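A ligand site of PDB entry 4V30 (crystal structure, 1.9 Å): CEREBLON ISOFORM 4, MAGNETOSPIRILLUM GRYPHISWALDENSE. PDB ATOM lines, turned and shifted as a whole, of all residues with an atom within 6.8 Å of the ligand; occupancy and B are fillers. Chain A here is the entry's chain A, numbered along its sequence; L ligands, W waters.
An oxygen (O1) of the ligand is in hydrogen-bond range of the side-chain amide nitrogen of Asn 51 (3.0 Å).
The backbone carbonyl oxygen (O) of Phe 78 is in hydrogen-bond range of a nitrogen (N1) of the ligand (2.9 Å).
O3 of the ligand is in hydrogen-bond range of OH of Tyr 102, at 2.8 Å.
An oxygen (O3) of the ligand lies within hydrogen-bond range of the backbone NH of Trp 80 (3.0 Å).
Pro 52 touches the ligand.
Ser 79 touches the ligand (CA to O3, 3.5 Å).
CE2 of Trp 86 touches C2 of the ligand, 3.5 Å away.
Trp 100 touches the ligand (NE1 to C2, 3.5 Å).
Hydrophobic or aromatic side chains that line the ligand: Pro 52, Phe 78, Trp 80, Trp 86, Trp 100 and Tyr 102.
The side-chain hydroxyl (OG) of Ser 79 sits at hydrogen-bond distance from the backbone carbonyl oxygen (O) of Phe 81 (3.2 Å).
O of Tyr 84 lies within hydrogen-bond range of OG of Ser 79 (2.8 Å).
OD1 of Asn 51 lies within hydrogen-bond range of N of Ala 53, 3.0 Å away.
O of Phe 50 sits at hydrogen-bond distance from NE1 of Trp 80.
N of Trp 86 is in hydrogen-bond range of O of Ser 75.
The indole nitrogen of Trp 86 sits at hydrogen-bond distance from the backbone carbonyl oxygen of Glu 77 (2.8 Å).
The side-chain amide oxygen (OD1) of Asn 51 is in hydrogen-bond range of the backbone NH (N) of Met 55 (3.1 Å).
Water W1 bridges NE1 of Trp 100 and O1 of the ligand.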
ATOM      1  N   VAL A  49      -7.394 -33.634  -1.899  1.00  0.00           N
ATOM      2  CA  VAL A  49      -6.404 -32.878  -1.096  1.00  0.00           C
ATOM      3  C   VAL A  49      -7.163 -32.221   0.082  1.00  0.00           C
ATOM      4  O   VAL A  49      -8.419 -32.014   0.012  1.00  0.00           O
ATOM      5  CB  VAL A  49      -5.698 -31.822  -1.999  1.00  0.00           C
ATOM      6  CG1 VAL A  49      -4.918 -32.536  -3.148  1.00  0.00           C
ATOM      7  CG2 VAL A  49      -6.722 -30.871  -2.552  1.00  0.00           C
ATOM      8  N   PHE A  50      -6.426 -31.826   1.115  1.00  0.00           N
ATOM      9  CA  PHE A  50      -6.999 -31.101   2.262  1.00  0.00           C
ATOM     10  C   PHE A  50      -6.212 -29.826   2.494  1.00  0.00           C
ATOM     11  O   PHE A  50      -5.009 -29.792   2.306  1.00  0.00           O
ATOM     12  CB  PHE A  50      -6.846 -31.935   3.539  1.00  0.00           C
ATOM     13  CG  PHE A  50      -7.498 -33.287   3.486  1.00  0.00           C
ATOM     14  CD1 PHE A  50      -6.805 -34.386   3.032  1.00  0.00           C
ATOM     15  CD2 PHE A  50      -8.782 -33.473   3.969  1.00  0.00           C
ATOM     16  CE1 PHE A  50      -7.405 -35.631   3.027  1.00  0.00           C
ATOM     17  CE2 PHE A  50      -9.393 -34.721   3.944  1.00  0.00           C
ATOM     18  CZ  PHE A  50      -8.695 -35.819   3.483  1.00  0.00           C
ATOM     19  N   ASN A  51      -6.897 -28.778   2.898  1.00  0.00           N
ATOM     20  CA  ASN A  51      -6.215 -27.507   3.218  1.00  0.00           C
ATOM     21  C   ASN A  51      -5.960 -27.486   4.764  1.00  0.00           C
ATOM     22  O   ASN A  51      -6.373 -28.398   5.478  1.00  0.00           O
ATOM     23  CB  ASN A  51      -7.026 -26.337   2.627  1.00  0.00           C
ATOM     24  CG  ASN A  51      -8.348 -26.148   3.318  1.00  0.00           C
ATOM     25  OD1 ASN A  51      -8.611 -26.749   4.371  1.00  0.00           O
ATOM     26  ND2 ASN A  51      -9.167 -25.321   2.744  1.00  0.00           N
ATOM     27  N   PRO A  52      -5.239 -26.462   5.273  1.00  0.00           N
ATOM     28  CA  PRO A  52      -4.979 -26.348   6.717  1.00  0.00           C
ATOM     29  C   PRO A  52      -6.229 -26.252   7.617  1.00  0.00           C
ATOM     30  O   PRO A  52      -6.136 -26.472   8.815  1.00  0.00           O
ATOM     31  CB  PRO A  52      -4.116 -25.076   6.817  1.00  0.00           C
ATOM     32  CG  PRO A  52      -3.510 -24.897   5.465  1.00  0.00           C
ATOM     33  CD  PRO A  52      -4.432 -25.534   4.473  1.00  0.00           C
ATOM     34  N   ALA A  53      -7.375 -25.940   7.038  1.00  0.00           N
ATOM     35  CA  ALA A  53      -8.657 -25.907   7.732  1.00  0.00           C
ATOM     36  C   ALA A  53      -9.395 -27.250   7.675  1.00  0.00           C
ATOM     37  O   ALA A  53     -10.540 -27.318   8.143  1.00  0.00           O
ATOM     38  CB  ALA A  53      -9.545 -24.817   7.176  1.00  0.00           C
ATOM     39  N   MET A  55     -10.599 -28.956   5.206  1.00  0.00           N
ATOM     40  CA  MET A  55     -11.530 -29.174   4.079  1.00  0.00           C
ATOM     41  C   MET A  55     -10.895 -30.109   3.033  1.00  0.00           C
ATOM     42  O   MET A  55      -9.738 -29.944   2.658  1.00  0.00           O
ATOM     43  CB  MET A  55     -11.952 -27.865   3.416  1.00  0.00           C
ATOM     44  CG  MET A  55     -12.498 -26.878   4.418  1.00  0.00           C
ATOM     45  SD  MET A  55     -12.879 -25.270   3.704  1.00  0.00           S
ATOM     46  CE  MET A  55     -13.329 -24.520   5.288  1.00  0.00           C
ATOM     47  N   PHE A  57     -11.126 -31.668  -0.814  1.00  0.00           N
ATOM     48  CA  PHE A  57     -11.479 -31.154  -2.142  1.00  0.00           C
ATOM     49  C   PHE A  57     -11.157 -32.260  -3.109  1.00  0.00           C
ATOM     50  O   PHE A  57     -10.038 -32.822  -3.080  1.00  0.00           O
ATOM     51  CB  PHE A  57     -10.678 -29.924  -2.512  1.00  0.00           C
ATOM     52  CG  PHE A  57     -10.932 -28.688  -1.626  1.00  0.00           C
ATOM     53  CD1 PHE A  57     -12.034 -27.927  -1.816  1.00  0.00           C
ATOM     54  CD2 PHE A  57     -10.035 -28.325  -0.618  1.00  0.00           C
ATOM     55  CE1 PHE A  57     -12.295 -26.818  -1.000  1.00  0.00           C
ATOM     56  CE2 PHE A  57     -10.278 -27.201   0.164  1.00  0.00           C
ATOM     57  CZ  PHE A  57     -11.404 -26.426  -0.051  1.00  0.00           C
ATOM     58  N   SER A  75       0.995 -17.558  -4.403  1.00  0.00           N
ATOM     59  CA  SER A  75       1.603 -17.967  -3.188  1.00  0.00           C
ATOM     60  C   SER A  75       2.015 -19.423  -3.404  1.00  0.00           C
ATOM     61  O   SER A  75       1.249 -20.202  -3.978  1.00  0.00           O
ATOM     62  CB  SER A  75       0.632 -17.848  -1.994  1.00  0.00           C
ATOM     63  OG  SER A  75       1.356 -18.291  -0.830  1.00  0.00           O
ATOM     64  N   GLY A  76       3.229 -19.781  -3.004  1.00  0.00           N
ATOM     65  CA  GLY A  76       3.675 -21.173  -2.906  1.00  0.00           C
ATOM     66  C   GLY A  76       3.237 -21.888  -1.634  1.00  0.00           C
ATOM     67  O   GLY A  76       3.359 -23.094  -1.544  1.00  0.00           O
ATOM     68  N   GLU A  77       2.730 -21.179  -0.637  1.00  0.00           N
ATOM     69  CA  GLU A  77       2.536 -21.780   0.684  1.00  0.00           C
ATOM     70  C   GLU A  77       1.431 -22.845   0.630  1.00  0.00           C
ATOM     71  O   GLU A  77       0.407 -22.626   0.089  1.00  0.00           O
ATOM     72  CB  GLU A  77       2.179 -20.703   1.697  1.00  0.00           C
ATOM     73  CG  GLU A  77       3.368 -19.791   1.946  1.00  0.00           C
ATOM     74  CD  GLU A  77       4.429 -20.430   2.804  1.00  0.00           C
ATOM     75  OE1 GLU A  77       4.139 -20.675   3.999  1.00  0.00           O
ATOM     76  OE2 GLU A  77       5.577 -20.671   2.305  1.00  0.00           O
ATOM     77  N   PHE A  78       1.716 -24.046   1.141  1.00  0.00           N
ATOM     78  CA  PHE A  78       0.742 -25.128   1.248  1.00  0.00           C
ATOM     79  C   PHE A  78       0.358 -25.685  -0.111  1.00  0.00           C
ATOM     80  O   PHE A  78      -0.653 -26.406  -0.223  1.00  0.00           O
ATOM     81  CB  PHE A  78      -0.528 -24.708   1.993  1.00  0.00           C
ATOM     82  CG  PHE A  78      -0.290 -24.260   3.412  1.00  0.00           C
ATOM     83  CD1 PHE A  78       0.139 -25.141   4.342  1.00  0.00           C
ATOM     84  CD2 PHE A  78      -0.507 -22.959   3.786  1.00  0.00           C
ATOM     85  CE1 PHE A  78       0.357 -24.750   5.646  1.00  0.00           C
ATOM     86  CE2 PHE A  78      -0.296 -22.539   5.089  1.00  0.00           C
ATOM     87  CZ  PHE A  78       0.100 -23.439   6.021  1.00  0.00           C
ATOM     88  N   SER A  79       1.105 -25.332  -1.150  1.00  0.00           N
ATOM     89  CA  SER A  79       0.746 -25.769  -2.465  1.00  0.00           C
ATOM     90  C   SER A  79       0.649 -27.290  -2.532  1.00  0.00           C
ATOM     91  O   SER A  79       1.561 -27.982  -2.080  1.00  0.00           O
ATOM     92  CB  SER A  79       1.691 -25.263  -3.513  1.00  0.00           C
ATOM     93  OG  SER A  79       1.191 -25.684  -4.806  1.00  0.00           O
ATOM     94  N   TRP A  80      -0.446 -27.802  -3.103  1.00  0.00           N
ATOM     95  CA  TRP A  80      -0.655 -29.250  -3.347  1.00  0.00           C
ATOM     96  C   TRP A  80       0.144 -29.784  -4.541  1.00  0.00           C
ATOM     97  O   TRP A  80       0.244 -30.989  -4.736  1.00  0.00           O
ATOM     98  CB  TRP A  80      -2.114 -29.581  -3.584  1.00  0.00           C
ATOM     99  CG  TRP A  80      -3.001 -29.297  -2.398  1.00  0.00           C
ATOM    100  CD1 TRP A  80      -2.786 -29.743  -1.110  1.00  0.00           C
ATOM    101  CD2 TRP A  80      -4.199 -28.569  -2.392  1.00  0.00           C
ATOM    102  NE1 TRP A  80      -3.783 -29.264  -0.282  1.00  0.00           N
ATOM    103  CE2 TRP A  80      -4.684 -28.573  -1.070  1.00  0.00           C
ATOM    104  CE3 TRP A  80      -4.894 -27.859  -3.369  1.00  0.00           C
ATOM    105  CZ2 TRP A  80      -5.819 -27.907  -0.703  1.00  0.00           C
ATOM    106  CZ3 TRP A  80      -6.052 -27.220  -3.032  1.00  0.00           C
ATOM    107  CH2 TRP A  80      -6.521 -27.261  -1.682  1.00  0.00           C
ATOM    108  N   PHE A  81       0.747 -28.908  -5.345  1.00  0.00           N
ATOM    109  CA  PHE A  81       1.392 -29.368  -6.576  1.00  0.00           C
ATOM    110  C   PHE A  81       2.787 -28.828  -6.549  1.00  0.00           C
ATOM    111  O   PHE A  81       2.976 -27.595  -6.621  1.00  0.00           O
ATOM    112  CB  PHE A  81       0.556 -28.872  -7.777  1.00  0.00           C
ATOM    113  CG  PHE A  81      -0.844 -29.444  -7.859  1.00  0.00           C
ATOM    114  CD1 PHE A  81      -1.088 -30.750  -8.423  1.00  0.00           C
ATOM    115  CD2 PHE A  81      -1.878 -28.782  -7.348  1.00  0.00           C
ATOM    116  CE1 PHE A  81      -2.386 -31.266  -8.458  1.00  0.00           C
ATOM    117  CE2 PHE A  81      -3.178 -29.287  -7.383  1.00  0.00           C
ATOM    118  CZ  PHE A  81      -3.445 -30.517  -7.961  1.00  0.00           C
ATOM    119  N   TYR A  84       4.524 -25.352  -8.029  1.00  0.00           N
ATOM    120  CA  TYR A  84       3.524 -24.372  -8.481  1.00  0.00           C
ATOM    121  C   TYR A  84       3.079 -23.512  -7.341  1.00  0.00           C
ATOM    122  O   TYR A  84       2.979 -23.967  -6.166  1.00  0.00           O
ATOM    123  CB  TYR A  84       2.280 -25.025  -9.106  1.00  0.00           C
ATOM    124  CG  TYR A  84       2.565 -25.906 -10.312  1.00  0.00           C
ATOM    125  CD1 TYR A  84       2.869 -27.261 -10.178  1.00  0.00           C
ATOM    126  CD2 TYR A  84       2.480 -25.406 -11.595  1.00  0.00           C
ATOM    127  CE1 TYR A  84       3.130 -28.075 -11.318  1.00  0.00           C
ATOM    128  CE2 TYR A  84       2.760 -26.153 -12.678  1.00  0.00           C
ATOM    129  CZ  TYR A  84       3.028 -27.517 -12.544  1.00  0.00           C
ATOM    130  OH  TYR A  84       3.293 -28.175 -13.695  1.00  0.00           O
ATOM    131  N   TRP A  86      -0.050 -20.744  -6.301  1.00  0.00           N
ATOM    132  CA  TRP A  86      -1.494 -20.659  -6.540  1.00  0.00           C
ATOM    133  C   TRP A  86      -2.081 -19.268  -6.311  1.00  0.00           C
ATOM    134  O   TRP A  86      -1.633 -18.546  -5.469  1.00  0.00           O
ATOM    135  CB  TRP A  86      -2.257 -21.678  -5.715  1.00  0.00           C
ATOM    136  CG  TRP A  86      -1.950 -21.635  -4.276  1.00  0.00           C
ATOM    137  CD1 TRP A  86      -1.021 -22.413  -3.591  1.00  0.00           C
ATOM    138  CD2 TRP A  86      -2.561 -20.788  -3.288  1.00  0.00           C
ATOM    139  NE1 TRP A  86      -0.990 -22.028  -2.296  1.00  0.00           N
ATOM    140  CE2 TRP A  86      -1.894 -21.027  -2.082  1.00  0.00           C
ATOM    141  CE3 TRP A  86      -3.550 -19.760  -3.346  1.00  0.00           C
ATOM    142  CZ2 TRP A  86      -2.221 -20.354  -0.896  1.00  0.00           C
ATOM    143  CZ3 TRP A  86      -3.871 -19.115  -2.161  1.00  0.00           C
ATOM    144  CH2 TRP A  86      -3.220 -19.431  -0.953  1.00  0.00           C
ATOM    145  N   THR A  87      -3.153 -19.022  -7.032  1.00  0.00           N
ATOM    146  CA  THR A  87      -4.099 -17.927  -6.734  1.00  0.00           C
ATOM    147  C   THR A  87      -5.454 -18.528  -6.722  1.00  0.00           C
ATOM    148  O   THR A  87      -5.816 -19.414  -7.535  1.00  0.00           O
ATOM    149  CB  THR A  87      -3.970 -16.886  -7.795  1.00  0.00           C
ATOM    150  OG1 THR A  87      -4.410 -17.435  -9.034  1.00  0.00           O
ATOM    151  CG2 THR A  87      -2.477 -16.499  -7.931  1.00  0.00           C
ATOM    152  N   ILE A  88      -6.241 -18.046  -5.788  1.00  0.00           N
ATOM    153  CA  ILE A  88      -7.666 -18.325  -5.761  1.00  0.00           C
ATOM    154  C   ILE A  88      -8.346 -17.945  -7.060  1.00  0.00           C
ATOM    155  O   ILE A  88      -8.122 -16.821  -7.589  1.00  0.00           O
ATOM    156  CB  ILE A  88      -8.324 -17.600  -4.558  1.00  0.00           C
ATOM    157  CG1 ILE A  88      -7.791 -18.265  -3.295  1.00  0.00           C
ATOM    158  CG2 ILE A  88      -9.852 -17.699  -4.615  1.00  0.00           C
ATOM    159  CD1 ILE A  88      -8.002 -17.448  -2.065  1.00  0.00           C
ATOM    160  N   HIS A  97     -16.304 -19.774  -5.107  1.00  0.00           N
ATOM    161  CA  HIS A  97     -14.948 -20.287  -5.161  1.00  0.00           C
ATOM    162  C   HIS A  97     -14.882 -21.579  -5.923  1.00  0.00           C
ATOM    163  O   HIS A  97     -15.403 -22.562  -5.463  1.00  0.00           O
ATOM    164  CB  HIS A  97     -14.446 -20.473  -3.742  1.00  0.00           C
ATOM    165  CG  HIS A  97     -13.050 -20.975  -3.711  1.00  0.00           C
ATOM    166  ND1 HIS A  97     -12.554 -21.714  -2.660  1.00  0.00           N
ATOM    167  CD2 HIS A  97     -12.076 -20.956  -4.646  1.00  0.00           C
ATOM    168  CE1 HIS A  97     -11.304 -22.040  -2.907  1.00  0.00           C
ATOM    169  NE2 HIS A  97     -11.008 -21.608  -4.130  1.00  0.00           N
ATOM    170  N   TRP A 100      -8.434 -23.023  -8.002  1.00  0.00           N
ATOM    171  CA  TRP A 100      -7.190 -22.305  -7.984  1.00  0.00           C
ATOM    172  C   TRP A 100      -6.568 -22.319  -9.377  1.00  0.00           C
ATOM    173  O   TRP A 100      -6.714 -23.263 -10.160  1.00  0.00           O
ATOM    174  CB  TRP A 100      -6.207 -22.900  -6.931  1.00  0.00           C
ATOM    175  CG  TRP A 100      -6.801 -22.951  -5.517  1.00  0.00           C
ATOM    176  CD1 TRP A 100      -6.675 -22.000  -4.556  1.00  0.00           C
ATOM    177  CD2 TRP A 100      -7.631 -23.970  -4.945  1.00  0.00           C
ATOM    178  NE1 TRP A 100      -7.418 -22.330  -3.476  1.00  0.00           N
ATOM    179  CE2 TRP A 100      -7.977 -23.568  -3.680  1.00  0.00           C
ATOM    180  CE3 TRP A 100      -8.120 -25.213  -5.403  1.00  0.00           C
ATOM    181  CZ2 TRP A 100      -8.813 -24.358  -2.853  1.00  0.00           C
ATOM    182  CZ3 TRP A 100      -8.952 -25.921  -4.633  1.00  0.00           C
ATOM    183  CH2 TRP A 100      -9.267 -25.542  -3.388  1.00  0.00           C
ATOM    184  N   TYR A 102      -2.800 -22.322 -11.020  1.00  0.00           N
ATOM    185  CA  TYR A 102      -1.402 -22.644 -10.654  1.00  0.00           C
ATOM    186  C   TYR A 102      -0.439 -22.176 -11.732  1.00  0.00           C
ATOM    187  O   TYR A 102      -0.744 -22.226 -12.910  1.00  0.00           O
ATOM    188  CB  TYR A 102      -1.289 -24.202 -10.466  1.00  0.00           C
ATOM    189  CG  TYR A 102      -1.968 -24.679  -9.202  1.00  0.00           C
ATOM    190  CD1 TYR A 102      -1.343 -24.692  -8.001  1.00  0.00           C
ATOM    191  CD2 TYR A 102      -3.305 -25.111  -9.248  1.00  0.00           C
ATOM    192  CE1 TYR A 102      -1.970 -25.136  -6.830  1.00  0.00           C
ATOM    193  CE2 TYR A 102      -3.995 -25.510  -8.110  1.00  0.00           C
ATOM    194  CZ  TYR A 102      -3.321 -25.573  -6.910  1.00  0.00           C
ATOM    195  OH  TYR A 102      -4.009 -25.992  -5.785  1.00  0.00           O
HETATM  196  C1  LIG L   1      -5.098 -24.090  -0.488  1.00  0.00           C
HETATM  197  C2  LIG L   1      -4.588 -23.200  -1.584  1.00  0.00           C
HETATM  198  C3  LIG L   1      -4.311 -24.134  -2.755  1.00  0.00           C
HETATM  199  C4  LIG L   1      -3.302 -25.206  -2.430  1.00  0.00           C
HETATM  200  N1  LIG L   1      -3.245 -25.641  -1.203  1.00  0.00           N
HETATM  201  C5  LIG L   1      -4.077 -25.190  -0.206  1.00  0.00           C
HETATM  202  C6  LIG L   1      -6.563 -22.609   2.599  1.00  0.00           C
HETATM  203  C7  LIG L   1      -5.247 -22.264   2.750  1.00  0.00           C
HETATM  204  C8  LIG L   1      -4.378 -22.727   1.645  1.00  0.00           C
HETATM  205  N2  LIG L   1      -5.380 -23.383   0.802  1.00  0.00           N
HETATM  206  C9  LIG L   1      -6.561 -23.315   1.326  1.00  0.00           C
HETATM  207  C10 LIG L   1      -7.218 -21.627   4.610  1.00  0.00           C
HETATM  208  C11 LIG L   1      -5.895 -21.279   4.861  1.00  0.00           C
HETATM  209  C12 LIG L   1      -4.901 -21.574   3.927  1.00  0.00           C
HETATM  210  C13 LIG L   1      -7.584 -22.300   3.494  1.00  0.00           C
HETATM  211  O1  LIG L   1      -7.680 -23.865   0.639  1.00  0.00           O
HETATM  212  N3  LIG L   1      -3.635 -21.208   4.240  1.00  0.00           N
HETATM  213  O2  LIG L   1      -3.977 -25.647   0.926  1.00  0.00           O
HETATM  214  O3  LIG L   1      -2.604 -25.679  -3.346  1.00  0.00           O
HETATM  215  O   HOH W   1      -7.440 -21.078  -0.858  1.00  0.00           O
HETATM  216  O   HOH W   2      -3.110 -19.475   2.577  1.00  0.00           O
